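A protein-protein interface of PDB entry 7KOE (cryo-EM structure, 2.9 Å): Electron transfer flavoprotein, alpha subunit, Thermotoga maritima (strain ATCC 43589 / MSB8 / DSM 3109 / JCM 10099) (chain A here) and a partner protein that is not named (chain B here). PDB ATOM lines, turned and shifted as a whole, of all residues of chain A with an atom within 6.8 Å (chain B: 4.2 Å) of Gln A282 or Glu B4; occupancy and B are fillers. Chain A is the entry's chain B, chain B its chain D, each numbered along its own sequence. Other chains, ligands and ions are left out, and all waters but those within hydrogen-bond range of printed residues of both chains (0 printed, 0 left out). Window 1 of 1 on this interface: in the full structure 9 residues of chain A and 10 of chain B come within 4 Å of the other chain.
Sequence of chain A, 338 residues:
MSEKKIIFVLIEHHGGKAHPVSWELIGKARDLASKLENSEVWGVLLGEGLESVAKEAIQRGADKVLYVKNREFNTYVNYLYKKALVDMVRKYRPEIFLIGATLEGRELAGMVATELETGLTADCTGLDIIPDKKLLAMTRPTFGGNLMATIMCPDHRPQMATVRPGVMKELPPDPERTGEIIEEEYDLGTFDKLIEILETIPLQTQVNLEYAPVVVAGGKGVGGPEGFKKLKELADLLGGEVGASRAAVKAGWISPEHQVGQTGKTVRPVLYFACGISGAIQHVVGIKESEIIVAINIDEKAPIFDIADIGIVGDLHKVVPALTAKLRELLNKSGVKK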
ATOM      1  N   VAL A 260      -0.345 -13.795  18.464  1.00  0.00           N
ATOM      2  CA  VAL A 260       0.481 -14.867  17.930  1.00  0.00           C
ATOM      3  C   VAL A 260       1.931 -14.556  18.267  1.00  0.00           C
ATOM      4  O   VAL A 260       2.404 -13.444  18.018  1.00  0.00           O
ATOM      5  CB  VAL A 260       0.291 -15.014  16.408  1.00  0.00           C
ATOM      6  CG1 VAL A 260       1.238 -16.041  15.845  1.00  0.00           C
ATOM      7  CG2 VAL A 260      -1.140 -15.387  16.087  1.00  0.00           C
ATOM      8  N   GLY A 261       2.628 -15.529  18.846  1.00  0.00           N
ATOM      9  CA  GLY A 261       4.047 -15.368  19.069  1.00  0.00           C
ATOM     10  C   GLY A 261       4.574 -16.101  20.281  1.00  0.00           C
ATOM     11  O   GLY A 261       4.131 -17.209  20.591  1.00  0.00           O
ATOM     12  N   GLN A 262       5.528 -15.479  20.975  1.00  0.00           N
ATOM     13  CA  GLN A 262       6.167 -16.124  22.116  1.00  0.00           C
ATOM     14  C   GLN A 262       5.233 -16.171  23.315  1.00  0.00           C
ATOM     15  O   GLN A 262       4.958 -17.243  23.863  1.00  0.00           O
ATOM     16  CB  GLN A 262       7.459 -15.391  22.466  1.00  0.00           C
ATOM     17  CG  GLN A 262       8.038 -15.772  23.801  1.00  0.00           C
ATOM     18  CD  GLN A 262       9.447 -15.283  23.964  1.00  0.00           C
ATOM     19  OE1 GLN A 262       9.680 -14.122  24.284  1.00  0.00           O
ATOM     20  NE2 GLN A 262      10.404 -16.168  23.740  1.00  0.00           N
ATOM     21  N   THR A 263       4.737 -15.012  23.742  1.00  0.00           N
ATOM     22  CA  THR A 263       3.801 -14.928  24.853  1.00  0.00           C
ATOM     23  C   THR A 263       2.358 -14.852  24.379  1.00  0.00           C
ATOM     24  O   THR A 263       1.488 -14.357  25.099  1.00  0.00           O
ATOM     25  CB  THR A 263       4.131 -13.734  25.743  1.00  0.00           C
ATOM     26  OG1 THR A 263       4.027 -12.526  24.983  1.00  0.00           O
ATOM     27  CG2 THR A 263       5.534 -13.860  26.296  1.00  0.00           C
ATOM     28  N   GLY A 264       2.092 -15.333  23.171  1.00  0.00           N
ATOM     29  CA  GLY A 264       0.741 -15.453  22.674  1.00  0.00           C
ATOM     30  C   GLY A 264       0.419 -16.903  22.390  1.00  0.00           C
ATOM     31  O   GLY A 264       0.530 -17.750  23.279  1.00  0.00           O
ATOM     32  N   GLY A 279       8.001  -8.839  11.833  1.00  0.00           N
ATOM     33  CA  GLY A 279       8.624 -10.140  11.896  1.00  0.00           C
ATOM     34  C   GLY A 279       9.766 -10.189  12.881  1.00  0.00           C
ATOM     35  O   GLY A 279      10.850 -10.687  12.565  1.00  0.00           O
ATOM     36  N   ALA A 280       9.538  -9.664  14.079  1.00  0.00           N
ATOM     37  CA  ALA A 280      10.515  -9.802  15.140  1.00  0.00           C
ATOM     38  C   ALA A 280      10.551 -11.241  15.633  1.00  0.00           C
ATOM     39  O   ALA A 280       9.626 -12.024  15.409  1.00  0.00           O
ATOM     40  CB  ALA A 280      10.197  -8.856  16.290  1.00  0.00           C
ATOM     41  N   ILE A 281      11.642 -11.579  16.324  1.00  0.00           N
ATOM     42  CA  ILE A 281      11.917 -12.963  16.695  1.00  0.00           C
ATOM     43  C   ILE A 281      10.925 -13.456  17.744  1.00  0.00           C
ATOM     44  O   ILE A 281      10.600 -14.648  17.793  1.00  0.00           O
ATOM     45  CB  ILE A 281      13.390 -13.066  17.144  1.00  0.00           C
ATOM     46  CG1 ILE A 281      13.771 -14.481  17.592  1.00  0.00           C
ATOM     47  CG2 ILE A 281      13.700 -12.032  18.208  1.00  0.00           C
ATOM     48  CD1 ILE A 281      13.591 -15.530  16.528  1.00  0.00           C
ATOM     49  N   GLN A 282      10.369 -12.551  18.546  1.00  0.00           N
ATOM     50  CA  GLN A 282       9.339 -12.944  19.496  1.00  0.00           C
ATOM     51  C   GLN A 282       8.013 -13.248  18.818  1.00  0.00           C
ATOM     52  O   GLN A 282       7.195 -13.973  19.389  1.00  0.00           O
ATOM     53  CB  GLN A 282       9.150 -11.856  20.544  1.00  0.00           C
ATOM     54  CG  GLN A 282      10.248 -11.801  21.573  1.00  0.00           C
ATOM     55  CD  GLN A 282      11.234 -10.697  21.299  1.00  0.00           C
ATOM     56  OE1 GLN A 282      11.102  -9.962  20.326  1.00  0.00           O
ATOM     57  NE2 GLN A 282      12.232 -10.570  22.157  1.00  0.00           N
ATOM     58  N   HIS A 283       7.780 -12.719  17.619  1.00  0.00           N
ATOM     59  CA  HIS A 283       6.570 -13.064  16.885  1.00  0.00           C
ATOM     60  C   HIS A 283       6.757 -14.286  15.998  1.00  0.00           C
ATOM     61  O   HIS A 283       5.911 -15.184  16.001  1.00  0.00           O
ATOM     62  CB  HIS A 283       6.100 -11.890  16.026  1.00  0.00           C
ATOM     63  CG  HIS A 283       4.847 -12.183  15.264  1.00  0.00           C
ATOM     64  ND1 HIS A 283       3.595 -12.068  15.824  1.00  0.00           N
ATOM     65  CD2 HIS A 283       4.654 -12.616  13.998  1.00  0.00           C
ATOM     66  CE1 HIS A 283       2.683 -12.404  14.930  1.00  0.00           C
ATOM     67  NE2 HIS A 283       3.301 -12.746  13.816  1.00  0.00           N
ATOM     68  N   VAL A 284       7.866 -14.353  15.252  1.00  0.00           N
ATOM     69  CA  VAL A 284       8.083 -15.447  14.307  1.00  0.00           C
ATOM     70  C   VAL A 284       8.448 -16.761  14.974  1.00  0.00           C
ATOM     71  O   VAL A 284       8.587 -17.772  14.277  1.00  0.00           O
ATOM     72  CB  VAL A 284       9.178 -15.108  13.278  1.00  0.00           C
ATOM     73  CG1 VAL A 284       8.897 -13.772  12.638  1.00  0.00           C
ATOM     74  CG2 VAL A 284      10.546 -15.122  13.920  1.00  0.00           C
ATOM     75  N   VAL A 285       8.598 -16.790  16.300  1.00  0.00           N
ATOM     76  CA  VAL A 285       8.799 -18.058  16.996  1.00  0.00           C
ATOM     77  C   VAL A 285       7.486 -18.804  17.175  1.00  0.00           C
ATOM     78  O   VAL A 285       7.488 -19.979  17.562  1.00  0.00           O
ATOM     79  CB  VAL A 285       9.509 -17.789  18.338  1.00  0.00           C
ATOM     80  CG1 VAL A 285       8.545 -17.229  19.359  1.00  0.00           C
ATOM     81  CG2 VAL A 285      10.263 -19.019  18.853  1.00  0.00           C
ATOM     82  N   GLY A 286       6.359 -18.170  16.875  1.00  0.00           N
ATOM     83  CA  GLY A 286       5.085 -18.852  16.931  1.00  0.00           C
ATOM     84  C   GLY A 286       4.561 -19.244  15.566  1.00  0.00           C
ATOM     85  O   GLY A 286       3.572 -19.972  15.471  1.00  0.00           O
ATOM     86  N   MET B   1      14.271  -3.979  16.483  1.00  0.00           N
ATOM     87  CA  MET B   1      14.872  -5.010  15.646  1.00  0.00           C
ATOM     88  C   MET B   1      16.244  -5.422  16.168  1.00  0.00           C
ATOM     89  O   MET B   1      16.520  -6.609  16.340  1.00  0.00           O
ATOM     90  CB  MET B   1      14.984  -4.525  14.197  1.00  0.00           C
ATOM     91  CG  MET B   1      15.946  -5.330  13.328  1.00  0.00           C
ATOM     92  SD  MET B   1      15.520  -7.079  13.199  1.00  0.00           S
ATOM     93  CE  MET B   1      17.133  -7.796  12.905  1.00  0.00           C
ATOM     94  N   ARG B   2      17.105  -4.435  16.419  1.00  0.00           N
ATOM     95  CA  ARG B   2      18.472  -4.739  16.821  1.00  0.00           C
ATOM     96  C   ARG B   2      18.533  -5.207  18.270  1.00  0.00           C
ATOM     97  O   ARG B   2      19.133  -6.244  18.570  1.00  0.00           O
ATOM     98  CB  ARG B   2      19.369  -3.520  16.601  1.00  0.00           C
ATOM     99  CG  ARG B   2      20.840  -3.740  16.945  1.00  0.00           C
ATOM    100  CD  ARG B   2      21.412  -4.990  16.284  1.00  0.00           C
ATOM    101  NE  ARG B   2      21.609  -6.064  17.253  1.00  0.00           N
ATOM    102  CZ  ARG B   2      21.774  -7.343  16.932  1.00  0.00           C
ATOM    103  NH1 ARG B   2      21.766  -7.714  15.660  1.00  0.00           N
ATOM    104  NH2 ARG B   2      21.944  -8.251  17.883  1.00  0.00           N
ATOM    105  N   ILE B   3      17.920  -4.458  19.189  1.00  0.00           N
ATOM    106  CA  ILE B   3      18.025  -4.840  20.592  1.00  0.00           C
ATOM    107  C   ILE B   3      16.981  -5.883  20.971  1.00  0.00           C
ATOM    108  O   ILE B   3      17.153  -6.580  21.977  1.00  0.00           O
ATOM    109  CB  ILE B   3      17.956  -3.605  21.509  1.00  0.00           C
ATOM    110  CG1 ILE B   3      18.740  -3.854  22.794  1.00  0.00           C
ATOM    111  CG2 ILE B   3      16.547  -3.287  21.900  1.00  0.00           C
ATOM    112  CD1 ILE B   3      20.191  -4.114  22.557  1.00  0.00           C
ATOM    113  N   GLU B   4      15.924  -6.052  20.179  1.00  0.00           N
ATOM    114  CA  GLU B   4      15.003  -7.145  20.452  1.00  0.00           C
ATOM    115  C   GLU B   4      15.546  -8.491  20.000  1.00  0.00           C
ATOM    116  O   GLU B   4      14.960  -9.522  20.339  1.00  0.00           O
ATOM    117  CB  GLU B   4      13.646  -6.863  19.809  1.00  0.00           C
ATOM    118  CG  GLU B   4      12.736  -5.990  20.674  1.00  0.00           C
ATOM    119  CD  GLU B   4      13.033  -4.496  20.589  1.00  0.00           C
ATOM    120  OE1 GLU B   4      14.009  -4.097  19.920  1.00  0.00           O
ATOM    121  OE2 GLU B   4      12.284  -3.713  21.212  1.00  0.00           O
ATOM    122  N   ASP B   5      16.643  -8.504  19.243  1.00  0.00           N
ATOM    123  CA  ASP B   5      17.427  -9.723  19.106  1.00  0.00           C
ATOM    124  C   ASP B   5      18.059 -10.112  20.433  1.00  0.00           C
ATOM    125  O   ASP B   5      18.120 -11.298  20.774  1.00  0.00           O
ATOM    126  CB  ASP B   5      18.510  -9.534  18.048  1.00  0.00           C
ATOM    127  CG  ASP B   5      17.950  -9.414  16.653  1.00  0.00           C
ATOM    128  OD1 ASP B   5      16.881 -10.002  16.386  1.00  0.00           O
ATOM    129  OD2 ASP B   5      18.582  -8.731  15.821  1.00  0.00           O
ATOM    130  N   LYS B   6      18.539  -9.125  21.194  1.00  0.00           N
ATOM    131  CA  LYS B   6      19.198  -9.407  22.463  1.00  0.00           C
ATOM    132  C   LYS B   6      18.210  -9.521  23.611  1.00  0.00           C
ATOM    133  O   LYS B   6      18.513 -10.171  24.615  1.00  0.00           O
ATOM    134  CB  LYS B   6      20.239  -8.333  22.767  1.00  0.00           C
ATOM    135  CG  LYS B   6      21.619  -8.682  22.249  1.00  0.00           C
ATOM    136  CD  LYS B   6      22.460  -7.452  21.999  1.00  0.00           C
ATOM    137  CE  LYS B   6      22.710  -6.691  23.276  1.00  0.00           C
ATOM    138  NZ  LYS B   6      23.768  -5.657  23.102  1.00  0.00           N
ATOM    139  N   LEU B   7      17.035  -8.905  23.492  1.00  0.00           N
ATOM    140  CA  LEU B   7      16.002  -9.103  24.498  1.00  0.00           C
ATOM    141  C   LEU B   7      15.349 -10.465  24.378  1.00  0.00           C
ATOM    142  O   LEU B   7      14.699 -10.911  25.326  1.00  0.00           O
ATOM    143  CB  LEU B   7      14.931  -8.023  24.393  1.00  0.00           C
ATOM    144  CG  LEU B   7      15.323  -6.602  24.772  1.00  0.00           C
ATOM    145  CD1 LEU B   7      14.085  -5.753  24.808  1.00  0.00           C
ATOM    146  CD2 LEU B   7      16.028  -6.577  26.102  1.00  0.00           C
ATOM    147  N   TYR B   8      15.493 -11.123  23.230  1.00  0.00           N
ATOM    148  CA  TYR B   8      15.016 -12.487  23.081  1.00  0.00           C
ATOM    149  C   TYR B   8      15.844 -13.468  23.896  1.00  0.00           C
ATOM    150  O   TYR B   8      15.346 -14.541  24.248  1.00  0.00           O
ATOM    151  CB  TYR B   8      15.024 -12.873  21.600  1.00  0.00           C
ATOM    152  CG  TYR B   8      14.455 -14.239  21.325  1.00  0.00           C
ATOM    153  CD1 TYR B   8      13.124 -14.521  21.589  1.00  0.00           C
ATOM    154  CD2 TYR B   8      15.254 -15.252  20.820  1.00  0.00           C
ATOM    155  CE1 TYR B   8      12.604 -15.769  21.350  1.00  0.00           C
ATOM    156  CE2 TYR B   8      14.741 -16.503  20.576  1.00  0.00           C
ATOM    157  CZ  TYR B   8      13.417 -16.755  20.847  1.00  0.00           C
ATOM    158  OH  TYR B   8      12.903 -18.004  20.608  1.00  0.00           O
ATOM    159  N   ALA B  44      16.412  -1.035  26.690  1.00  0.00           N
ATOM    160  CA  ALA B  44      15.633  -2.124  26.122  1.00  0.00           C
ATOM    161  C   ALA B  44      14.721  -1.661  24.997  1.00  0.00           C
ATOM    162  O   ALA B  44      13.895  -2.452  24.535  1.00  0.00           O
ATOM    163  CB  ALA B  44      14.809  -2.811  27.204  1.00  0.00           C
ATOM    164  N   ASP B  45      14.862  -0.406  24.556  1.00  0.00           N
ATOM    165  CA  ASP B  45      14.065   0.229  23.507  1.00  0.00           C
ATOM    166  C   ASP B  45      12.573   0.127  23.777  1.00  0.00           C
ATOM    167  O   ASP B  45      11.789  -0.140  22.863  1.00  0.00           O
ATOM    168  CB  ASP B  45      14.388  -0.365  22.138  1.00  0.00           C
ATOM    169  CG  ASP B  45      15.408   0.445  21.381  1.00  0.00           C
ATOM    170  OD1 ASP B  45      15.375   1.686  21.492  1.00  0.00           O
ATOM    171  OD2 ASP B  45      16.246  -0.152  20.679  1.00  0.00           O
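The backbone carbonyl oxygen (O) of Gln A282 sits at hydrogen-bond distance from the backbone NH (N) of Gln A262 (2.7 Å).
The backbone NH (N) of Met B1 sits at hydrogen-bond distance from the side-chain carboxylate (OE1) of Glu B4 (3.4 Å).
The side-chain amide nitrogen of Gln A282 lies within hydrogen-bond range of the backbone carbonyl oxygen of Glu B4.
The side-chain amide nitrogen (NE2) of Gln A282 sits close to the backbone NH (N) of Tyr B8 (3.5 Å).
Among the printed residues, pairs that only touch across the chains: Gln A262 with Tyr B8 (3.3 Å), Val A285 with Tyr B8 (3.3 Å), Ile A281 with Glu B4 (3.5 Å), Ile A281 with Tyr B8 (3.6 Å) and Gln A282 with Leu B7 (3.8 Å).
Val A260 touches none of the printed residues of chain B.
Gln A282 touches three residues of chain B.
Of the printed residues of chain B, Val A285 touches Tyr B8.
Glu B4 touches two residues of chain A.
Asp B5 touches none of the printed residues of chain A.
Of the printed residues of chain A, Leu B7 touches Gln A282 (3.8 Å).
The nearest printed residue of chain B that does not touch Gln A282 is Asp B5 (5.7 Å).
The nearest residue of chain A that does not touch Glu B4 is Ala A280 (5.3 Å).
The nearest printed residue of chain A that does not touch Leu B7 is Gln A262 (6.0 Å).
Of the 13 printed residues of chain A, 4 touch a printed residue of chain B.
Hydrophobic or aromatic side chains of chain A that line the printed part of chain B: Ile A281 and Val A285.
Among the printed residues, no Asp or Glu carboxylate lies within 4 Å of a Lys or Arg side-chain nitrogen of the other chain.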
